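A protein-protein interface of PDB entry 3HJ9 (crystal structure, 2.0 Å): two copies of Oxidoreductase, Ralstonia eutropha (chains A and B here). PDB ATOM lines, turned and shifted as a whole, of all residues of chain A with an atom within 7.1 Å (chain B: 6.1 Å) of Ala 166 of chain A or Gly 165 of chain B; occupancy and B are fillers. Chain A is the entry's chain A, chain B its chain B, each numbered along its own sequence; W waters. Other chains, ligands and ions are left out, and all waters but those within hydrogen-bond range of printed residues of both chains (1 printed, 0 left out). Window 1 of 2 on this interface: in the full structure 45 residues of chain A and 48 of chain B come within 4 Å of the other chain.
The side-chain amide oxygen (OD1) of Asn 170 of chain A sits close to the side-chain carboxylate (OE2) of Glu 169 of chain B (2.6 Å).
O of Thr 84 of chain A sits close to OE2 of Glu 169 of chain B, 3.3 Å away.
OE2 of Glu 169 of chain A sits close to OD1 of Asn 170 of chain B, 2.6 Å away.
The side-chain hydroxyl (OG1) of Thr 84 of chain A lies within hydrogen-bond range of the backbone carbonyl oxygen (O) of Ala 71 of chain A, at 2.7 Å.
The backbone carbonyl oxygen (O) of Thr 84 of chain A lies within hydrogen-bond range of the side-chain amide nitrogen (ND2) of Asn 170 of chain A, at 3.2 Å.
The backbone carbonyl oxygen of Leu 207 of chain A is in hydrogen-bond range of the backbone NH of Phe 141 of chain A (2.8 Å).
O of Ala 71 of chain A is in hydrogen-bond range of ND2 of Asn 170 of chain A (3.0 Å).
Among the printed residues, pairs that only touch across the chains: Pro 86 of chain A with Glu 169 of chain B (3.2 Å), Ala 161 of chain A with Ala 162 of chain B (3.3 Å), Ala 162 of chain A with Ala 161 of chain B (3.4 Å), Ala 166 of chain A with Glu 169 of chain B (3.4 Å), Glu 169 of chain A with Ala 166 of chain B (3.4 Å), Ala 162 of chain A with Gly 165 of chain B (3.5 Å), Leu 173 of chain A with Asn 170 of chain B (3.5 Å), Thr 158 of chain A with Ala 161 of chain B (3.5 Å), Gly 165 of chain A with Ala 162 of chain B (3.6 Å), Ala 161 of chain A with Ala 161 of chain B (3.6 Å), Gly 165 of chain A with Ala 166 of chain B (3.7 Å), Ala 166 of chain A with Gly 165 of chain B (3.8 Å), Leu 207 of chain A with Ala 162 of chain B (3.97 Å) and Ala 162 of chain A with Leu 207 of chain B (3.97 Å).
Of the printed residues of chain B, Ala 166 of chain A touches Gly 165 and Glu 169.
Printed residues of chain B within 4 Å of Thr 158 of chain A: Ala 161.
Of the printed residues of chain A, Asn 170 of chain B touches Glu 169 (2.6 Å) and Leu 173 (3.5 Å).
Of the printed residues of chain B, Ala 161 of chain A touches Ala 161 and Ala 162.
Printed residues of chain B within 4 Å of Glu 169 of chain A: Ala 166 (3.4 Å) and Asn 170 (2.6 Å).
Printed residues of chain B within 4 Å of Leu 173 of chain A: Asn 170.
Ala 164 of chain B touches none of the printed residues of chain A.
The nearest printed residue of chain B that does not touch Ala 166 of chain A is Ala 166 of chain B (4.002 Å).
Printed residues of chain B that touch a printed residue of chain A: Ala 161, Ala 162, Gly 165, Ala 166, Glu 169, Asn 170 and Leu 207.
Hydrophobic or aromatic side chains of chain B that line the printed part of chain A: Ala 161, Ala 162, Ala 166 and Leu 207.
Printed residues of chain A that touch a printed residue of chain B: Thr 84, Pro 86, Thr 158, Ala 161, Ala 162, Gly 165, Ala 166, Glu 169, Asn 170, Leu 173 and Leu 207.
Hydrophobic or aromatic side chains of chain A that line the printed part of chain B: Pro 86, Ala 161, Ala 162, Ala 166, Leu 173 and Leu 207.
Among the printed residues, no Asp or Glu carboxylate lies within 4 Å of a Lys or Arg side-chain nitrogen of the other chain.
Ala 161 of chain B touches its own counterpart, Ala 161 of chain A.
Ala 162 of chain A touches Leu 207 of chain B, and with the chains exchanged Leu 207 of chain A touches Ala 162 of chain B.
Gly 165 of chain A touches Ala 166 of chain B, and with the chains exchanged Ala 166 of chain A touches Gly 165 of chain B.
Glu 169 of chain A touches Asn 170 of chain B, and with the chains exchanged Asn 170 of chain A touches Glu 169 of chain B.
Water W1 bridges the side-chain hydroxyl of Ser 160 of chain B and the side-chain hydroxyl of Thr 158 of chain A.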
ATOM      1  N   ALA A  71     -22.072  13.583  32.986  1.00  0.00           N
ATOM      2  CA  ALA A  71     -22.014  13.446  31.532  1.00  0.00           C
ATOM      3  C   ALA A  71     -22.101  14.846  30.909  1.00  0.00           C
ATOM      4  O   ALA A  71     -21.180  15.250  30.173  1.00  0.00           O
ATOM      5  CB  ALA A  71     -23.127  12.507  30.988  1.00  0.00           C
ATOM      6  N   ALA A  72     -23.103  15.625  31.324  1.00  0.00           N
ATOM      7  CA  ALA A  72     -23.315  16.985  30.759  1.00  0.00           C
ATOM      8  C   ALA A  72     -22.246  18.020  31.108  1.00  0.00           C
ATOM      9  O   ALA A  72     -21.756  18.741  30.206  1.00  0.00           O
ATOM     10  CB  ALA A  72     -24.705  17.521  31.132  1.00  0.00           C
ATOM     11  N   THR A  84     -16.177  17.200  30.718  1.00  0.00           N
ATOM     12  CA  THR A  84     -16.628  16.198  29.760  1.00  0.00           C
ATOM     13  C   THR A  84     -16.986  16.810  28.414  1.00  0.00           C
ATOM     14  O   THR A  84     -17.021  16.077  27.451  1.00  0.00           O
ATOM     15  CB  THR A  84     -17.859  15.427  30.291  1.00  0.00           C
ATOM     16  OG1 THR A  84     -18.824  16.392  30.684  1.00  0.00           O
ATOM     17  CG2 THR A  84     -17.468  14.525  31.514  1.00  0.00           C
ATOM     18  N   ALA A  85     -17.218  18.134  28.357  1.00  0.00           N
ATOM     19  CA  ALA A  85     -17.583  18.881  27.137  1.00  0.00           C
ATOM     20  C   ALA A  85     -16.609  20.055  26.963  1.00  0.00           C
ATOM     21  O   ALA A  85     -16.098  20.618  27.956  1.00  0.00           O
ATOM     22  CB  ALA A  85     -19.030  19.387  27.225  1.00  0.00           C
ATOM     23  N   PRO A  86     -16.330  20.429  25.709  1.00  0.00           N
ATOM     24  CA  PRO A  86     -15.427  21.552  25.478  1.00  0.00           C
ATOM     25  C   PRO A  86     -16.056  22.910  25.838  1.00  0.00           C
ATOM     26  O   PRO A  86     -17.269  23.023  26.080  1.00  0.00           O
ATOM     27  CB  PRO A  86     -15.149  21.454  23.982  1.00  0.00           C
ATOM     28  CG  PRO A  86     -16.458  20.899  23.441  1.00  0.00           C
ATOM     29  CD  PRO A  86     -16.906  19.921  24.449  1.00  0.00           C
ATOM     30  N   PHE A 141     -29.257  25.222  30.451  1.00  0.00           N
ATOM     31  CA  PHE A 141     -27.854  25.555  30.138  1.00  0.00           C
ATOM     32  C   PHE A 141     -27.811  27.078  30.078  1.00  0.00           C
ATOM     33  O   PHE A 141     -28.386  27.687  29.161  1.00  0.00           O
ATOM     34  CB  PHE A 141     -27.421  24.894  28.830  1.00  0.00           C
ATOM     35  CG  PHE A 141     -27.497  23.375  28.864  1.00  0.00           C
ATOM     36  CD1 PHE A 141     -28.668  22.717  28.541  1.00  0.00           C
ATOM     37  CD2 PHE A 141     -26.381  22.611  29.236  1.00  0.00           C
ATOM     38  CE1 PHE A 141     -28.749  21.319  28.590  1.00  0.00           C
ATOM     39  CE2 PHE A 141     -26.437  21.209  29.267  1.00  0.00           C
ATOM     40  CZ  PHE A 141     -27.615  20.562  28.934  1.00  0.00           C
ATOM     41  N   THR A 158     -22.708  32.106  19.246  1.00  0.00           N
ATOM     42  CA  THR A 158     -22.245  30.846  18.630  1.00  0.00           C
ATOM     43  C   THR A 158     -21.480  29.966  19.650  1.00  0.00           C
ATOM     44  O   THR A 158     -21.718  28.769  19.748  1.00  0.00           O
ATOM     45  CB  THR A 158     -21.331  31.087  17.431  1.00  0.00           C
ATOM     46  OG1 THR A 158     -22.025  31.871  16.447  1.00  0.00           O
ATOM     47  CG2 THR A 158     -20.870  29.761  16.799  1.00  0.00           C
ATOM     48  N   SER A 160     -21.513  30.095  23.044  1.00  0.00           N
ATOM     49  CA  SER A 160     -22.455  29.677  24.105  1.00  0.00           C
ATOM     50  C   SER A 160     -23.346  28.534  23.656  1.00  0.00           C
ATOM     51  O   SER A 160     -23.456  27.518  24.342  1.00  0.00           O
ATOM     52  CB  SER A 160     -23.385  30.818  24.498  1.00  0.00           C
ATOM     53  OG  SER A 160     -22.652  31.885  25.010  1.00  0.00           O
ATOM     54  N   ALA A 161     -23.977  28.714  22.487  1.00  0.00           N
ATOM     55  CA  ALA A 161     -24.905  27.714  21.896  1.00  0.00           C
ATOM     56  C   ALA A 161     -24.185  26.400  21.544  1.00  0.00           C
ATOM     57  O   ALA A 161     -24.726  25.345  21.805  1.00  0.00           O
ATOM     58  CB  ALA A 161     -25.628  28.293  20.631  1.00  0.00           C
ATOM     59  N   ALA A 162     -22.967  26.476  20.989  1.00  0.00           N
ATOM     60  CA  ALA A 162     -22.163  25.275  20.645  1.00  0.00           C
ATOM     61  C   ALA A 162     -21.760  24.477  21.890  1.00  0.00           C
ATOM     62  O   ALA A 162     -21.967  23.243  21.931  1.00  0.00           O
ATOM     63  CB  ALA A 162     -20.913  25.633  19.821  1.00  0.00           C
ATOM     64  N   ALA A 163     -21.241  25.188  22.904  1.00  0.00           N
ATOM     65  CA  ALA A 163     -20.888  24.612  24.230  1.00  0.00           C
ATOM     66  C   ALA A 163     -22.117  23.968  24.857  1.00  0.00           C
ATOM     67  O   ALA A 163     -22.049  22.799  25.233  1.00  0.00           O
ATOM     68  CB  ALA A 163     -20.309  25.693  25.178  1.00  0.00           C
ATOM     69  N   ALA A 164     -23.237  24.703  24.923  1.00  0.00           N
ATOM     70  CA  ALA A 164     -24.507  24.143  25.433  1.00  0.00           C
ATOM     71  C   ALA A 164     -25.000  22.910  24.619  1.00  0.00           C
ATOM     72  O   ALA A 164     -25.432  21.898  25.206  1.00  0.00           O
ATOM     73  CB  ALA A 164     -25.587  25.205  25.541  1.00  0.00           C
ATOM     74  N   GLY A 165     -24.851  22.982  23.289  1.00  0.00           N
ATOM     75  CA  GLY A 165     -25.178  21.878  22.410  1.00  0.00           C
ATOM     76  C   GLY A 165     -24.385  20.605  22.686  1.00  0.00           C
ATOM     77  O   GLY A 165     -24.927  19.517  22.662  1.00  0.00           O
ATOM     78  N   ALA A 166     -23.079  20.763  22.886  1.00  0.00           N
ATOM     79  CA  ALA A 166     -22.166  19.661  23.191  1.00  0.00           C
ATOM     80  C   ALA A 166     -22.535  19.022  24.503  1.00  0.00           C
ATOM     81  O   ALA A 166     -22.598  17.803  24.602  1.00  0.00           O
ATOM     82  CB  ALA A 166     -20.751  20.149  23.249  1.00  0.00           C
ATOM     83  N   MET A 167     -22.835  19.856  25.494  1.00  0.00           N
ATOM     84  CA  MET A 167     -23.184  19.376  26.830  1.00  0.00           C
ATOM     85  C   MET A 167     -24.531  18.676  26.807  1.00  0.00           C
ATOM     86  O   MET A 167     -24.705  17.600  27.418  1.00  0.00           O
ATOM     87  CB  MET A 167     -23.209  20.526  27.832  1.00  0.00           C
ATOM     88  CG  MET A 167     -21.855  21.153  27.971  1.00  0.00           C
ATOM     89  SD  MET A 167     -21.979  22.919  28.776  1.00  0.00           S
ATOM     90  CE  MET A 167     -21.690  22.468  30.602  1.00  0.00           C
ATOM     91  N   ALA A 168     -25.466  19.269  26.075  1.00  0.00           N
ATOM     92  CA  ALA A 168     -26.797  18.643  25.869  1.00  0.00           C
ATOM     93  C   ALA A 168     -26.621  17.337  25.079  1.00  0.00           C
ATOM     94  O   ALA A 168     -27.389  16.397  25.292  1.00  0.00           O
ATOM     95  CB  ALA A 168     -27.743  19.587  25.119  1.00  0.00           C
ATOM     96  N   GLU A 169     -25.606  17.256  24.186  1.00  0.00           N
ATOM     97  CA  GLU A 169     -25.384  16.011  23.425  1.00  0.00           C
ATOM     98  C   GLU A 169     -24.849  14.890  24.323  1.00  0.00           C
ATOM     99  O   GLU A 169     -25.264  13.738  24.189  1.00  0.00           O
ATOM    100  CB  GLU A 169     -24.480  16.234  22.206  1.00  0.00           C
ATOM    101  CG  GLU A 169     -24.354  15.041  21.285  1.00  0.00           C
ATOM    102  CD  GLU A 169     -25.663  14.591  20.633  1.00  0.00           C
ATOM    103  OE1 GLU A 169     -26.719  15.240  20.836  1.00  0.00           O
ATOM    104  OE2 GLU A 169     -25.624  13.569  19.891  1.00  0.00           O
ATOM    105  N   ASN A 170     -23.919  15.223  25.225  1.00  0.00           N
ATOM    106  CA  ASN A 170     -23.466  14.266  26.222  1.00  0.00           C
ATOM    107  C   ASN A 170     -24.672  13.715  27.005  1.00  0.00           C
ATOM    108  O   ASN A 170     -24.730  12.521  27.272  1.00  0.00           O
ATOM    109  CB  ASN A 170     -22.485  14.887  27.226  1.00  0.00           C
ATOM    110  CG  ASN A 170     -21.116  15.160  26.639  1.00  0.00           C
ATOM    111  OD1 ASN A 170     -20.833  14.797  25.495  1.00  0.00           O
ATOM    112  ND2 ASN A 170     -20.257  15.834  27.423  1.00  0.00           N
ATOM    113  N   ALA A 171     -25.603  14.595  27.370  1.00  0.00           N
ATOM    114  CA  ALA A 171     -26.828  14.203  28.140  1.00  0.00           C
ATOM    115  C   ALA A 171     -27.731  13.271  27.334  1.00  0.00           C
ATOM    116  O   ALA A 171     -28.283  12.289  27.881  1.00  0.00           O
ATOM    117  CB  ALA A 171     -27.617  15.461  28.629  1.00  0.00           C
ATOM    118  N   TYR A 172     -27.945  13.611  26.060  1.00  0.00           N
ATOM    119  CA  TYR A 172     -28.686  12.731  25.122  1.00  0.00           C
ATOM    120  C   TYR A 172     -28.140  11.316  25.047  1.00  0.00           C
ATOM    121  O   TYR A 172     -28.893  10.345  25.152  1.00  0.00           O
ATOM    122  CB  TYR A 172     -28.671  13.285  23.699  1.00  0.00           C
ATOM    123  CG  TYR A 172     -29.842  14.107  23.246  1.00  0.00           C
ATOM    124  CD1 TYR A 172     -31.098  13.528  23.064  1.00  0.00           C
ATOM    125  CD2 TYR A 172     -29.675  15.452  22.875  1.00  0.00           C
ATOM    126  CE1 TYR A 172     -32.199  14.309  22.551  1.00  0.00           C
ATOM    127  CE2 TYR A 172     -30.750  16.206  22.357  1.00  0.00           C
ATOM    128  CZ  TYR A 172     -31.983  15.652  22.201  1.00  0.00           C
ATOM    129  OH  TYR A 172     -32.988  16.437  21.684  1.00  0.00           O
ATOM    130  N   LEU A 173     -26.825  11.233  24.846  1.00  0.00           N
ATOM    131  CA  LEU A 173     -26.099   9.969  24.747  1.00  0.00           C
ATOM    132  C   LEU A 173     -26.174   9.188  26.067  1.00  0.00           C
ATOM    133  O   LEU A 173     -26.433   7.963  26.050  1.00  0.00           O
ATOM    134  CB  LEU A 173     -24.638  10.183  24.266  1.00  0.00           C
ATOM    135  CG  LEU A 173     -24.498  10.698  22.815  1.00  0.00           C
ATOM    136  CD1 LEU A 173     -23.065  11.129  22.484  1.00  0.00           C
ATOM    137  CD2 LEU A 173     -25.036   9.682  21.774  1.00  0.00           C
ATOM    138  N   LEU A 207     -30.408  27.010  26.268  1.00  0.00           N
ATOM    139  CA  LEU A 207     -31.174  25.812  25.946  1.00  0.00           C
ATOM    140  C   LEU A 207     -31.653  25.164  27.220  1.00  0.00           C
ATOM    141  O   LEU A 207     -31.035  25.340  28.276  1.00  0.00           O
ATOM    142  CB  LEU A 207     -30.277  24.766  25.255  1.00  0.00           C
ATOM    143  CG  LEU A 207     -29.614  25.037  23.923  1.00  0.00           C
ATOM    144  CD1 LEU A 207     -28.579  23.906  23.631  1.00  0.00           C
ATOM    145  CD2 LEU A 207     -30.663  25.177  22.794  1.00  0.00           C
ATOM    146  N   SER B 160     -28.336  26.665  14.771  1.00  0.00           N
ATOM    147  CA  SER B 160     -27.261  26.078  13.954  1.00  0.00           C
ATOM    148  C   SER B 160     -26.020  25.828  14.811  1.00  0.00           C
ATOM    149  O   SER B 160     -25.436  24.763  14.718  1.00  0.00           O
ATOM    150  CB  SER B 160     -26.946  26.936  12.740  1.00  0.00           C
ATOM    151  OG  SER B 160     -26.496  28.200  13.145  1.00  0.00           O
ATOM    152  N   ALA B 161     -25.666  26.770  15.685  1.00  0.00           N
ATOM    153  CA  ALA B 161     -24.521  26.583  16.598  1.00  0.00           C
ATOM    154  C   ALA B 161     -24.714  25.419  17.576  1.00  0.00           C
ATOM    155  O   ALA B 161     -23.771  24.617  17.768  1.00  0.00           O
ATOM    156  CB  ALA B 161     -24.172  27.899  17.347  1.00  0.00           C
ATOM    157  N   ALA B 162     -25.919  25.287  18.156  1.00  0.00           N
ATOM    158  CA  ALA B 162     -26.213  24.173  19.077  1.00  0.00           C
ATOM    159  C   ALA B 162     -26.202  22.809  18.338  1.00  0.00           C
ATOM    160  O   ALA B 162     -25.687  21.820  18.878  1.00  0.00           O
ATOM    161  CB  ALA B 162     -27.546  24.382  19.826  1.00  0.00           C
ATOM    162  N   ALA B 163     -26.731  22.783  17.100  1.00  0.00           N
ATOM    163  CA  ALA B 163     -26.705  21.574  16.259  1.00  0.00           C
ATOM    164  C   ALA B 163     -25.244  21.221  15.922  1.00  0.00           C
ATOM    165  O   ALA B 163     -24.845  20.053  16.069  1.00  0.00           O
ATOM    166  CB  ALA B 163     -27.552  21.760  14.949  1.00  0.00           C
ATOM    167  N   ALA B 164     -24.463  22.218  15.495  1.00  0.00           N
ATOM    168  CA  ALA B 164     -23.031  21.991  15.173  1.00  0.00           C
ATOM    169  C   ALA B 164     -22.210  21.524  16.382  1.00  0.00           C
ATOM    170  O   ALA B 164     -21.330  20.679  16.224  1.00  0.00           O
ATOM    171  CB  ALA B 164     -22.366  23.254  14.555  1.00  0.00           C
ATOM    172  N   GLY B 165     -22.460  22.120  17.553  1.00  0.00           N
ATOM    173  CA  GLY B 165     -21.789  21.732  18.787  1.00  0.00           C
ATOM    174  C   GLY B 165     -22.072  20.274  19.154  1.00  0.00           C
ATOM    175  O   GLY B 165     -21.163  19.554  19.565  1.00  0.00           O
ATOM    176  N   ALA B 166     -23.342  19.851  18.998  1.00  0.00           N
ATOM    177  CA  ALA B 166     -23.724  18.444  19.249  1.00  0.00           C
ATOM    178  C   ALA B 166     -23.046  17.463  18.282  1.00  0.00           C
ATOM    179  O   ALA B 166     -22.575  16.400  18.669  1.00  0.00           O
ATOM    180  CB  ALA B 166     -25.256  18.270  19.210  1.00  0.00           C
ATOM    181  N   MET B 167     -22.976  17.837  17.028  1.00  0.00           N
ATOM    182  CA  MET B 167     -22.326  17.011  16.010  1.00  0.00           C
ATOM    183  C   MET B 167     -20.834  16.893  16.278  1.00  0.00           C
ATOM    184  O   MET B 167     -20.288  15.782  16.280  1.00  0.00           O
ATOM    185  CB  MET B 167     -22.633  17.574  14.625  1.00  0.00           C
ATOM    186  CG  MET B 167     -24.128  17.541  14.307  1.00  0.00           C
ATOM    187  SD  MET B 167     -24.583  18.801  12.894  1.00  0.00           S
ATOM    188  CE  MET B 167     -23.937  17.731  11.463  1.00  0.00           C
ATOM    189  N   ALA B 168     -20.191  18.033  16.565  1.00  0.00           N
ATOM    190  CA  ALA B 168     -18.745  18.048  16.906  1.00  0.00           C
ATOM    191  C   ALA B 168     -18.485  17.232  18.197  1.00  0.00           C
ATOM    192  O   ALA B 168     -17.406  16.643  18.338  1.00  0.00           O
ATOM    193  CB  ALA B 168     -18.231  19.463  17.090  1.00  0.00           C
ATOM    194  N   GLU B 169     -19.468  17.225  19.107  1.00  0.00           N
ATOM    195  CA  GLU B 169     -19.373  16.474  20.359  1.00  0.00           C
ATOM    196  C   GLU B 169     -19.437  14.979  20.067  1.00  0.00           C
ATOM    197  O   GLU B 169     -18.621  14.224  20.618  1.00  0.00           O
ATOM    198  CB  GLU B 169     -20.426  16.876  21.397  1.00  0.00           C
ATOM    199  CG  GLU B 169     -20.271  16.182  22.779  1.00  0.00           C
ATOM    200  CD  GLU B 169     -18.964  16.520  23.517  1.00  0.00           C
ATOM    201  OE1 GLU B 169     -18.228  17.416  23.048  1.00  0.00           O
ATOM    202  OE2 GLU B 169     -18.677  15.910  24.594  1.00  0.00           O
ATOM    203  N   ASN B 170     -20.381  14.554  19.223  1.00  0.00           N
ATOM    204  CA  ASN B 170     -20.422  13.137  18.818  1.00  0.00           C
ATOM    205  C   ASN B 170     -19.027  12.748  18.252  1.00  0.00           C
ATOM    206  O   ASN B 170     -18.494  11.702  18.594  1.00  0.00           O
ATOM    207  CB  ASN B 170     -21.465  12.885  17.748  1.00  0.00           C
ATOM    208  CG  ASN B 170     -22.890  12.887  18.255  1.00  0.00           C
ATOM    209  OD1 ASN B 170     -23.134  12.906  19.434  1.00  0.00           O
ATOM    210  ND2 ASN B 170     -23.848  12.797  17.315  1.00  0.00           N
ATOM    211  N   LEU B 207     -18.152  26.245  12.793  1.00  0.00           N
ATOM    212  CA  LEU B 207     -17.162  25.511  13.575  1.00  0.00           C
ATOM    213  C   LEU B 207     -16.341  24.634  12.631  1.00  0.00           C
ATOM    214  O   LEU B 207     -16.855  24.183  11.591  1.00  0.00           O
ATOM    215  CB  LEU B 207     -17.829  24.611  14.638  1.00  0.00           C
ATOM    216  CG  LEU B 207     -18.717  25.179  15.745  1.00  0.00           C
ATOM    217  CD1 LEU B 207     -19.436  24.032  16.497  1.00  0.00           C
ATOM    218  CD2 LEU B 207     -17.931  26.051  16.704  1.00  0.00           C
HETATM  219  O   HOH W   1     -24.283  30.032  14.769  1.00  0.00           O
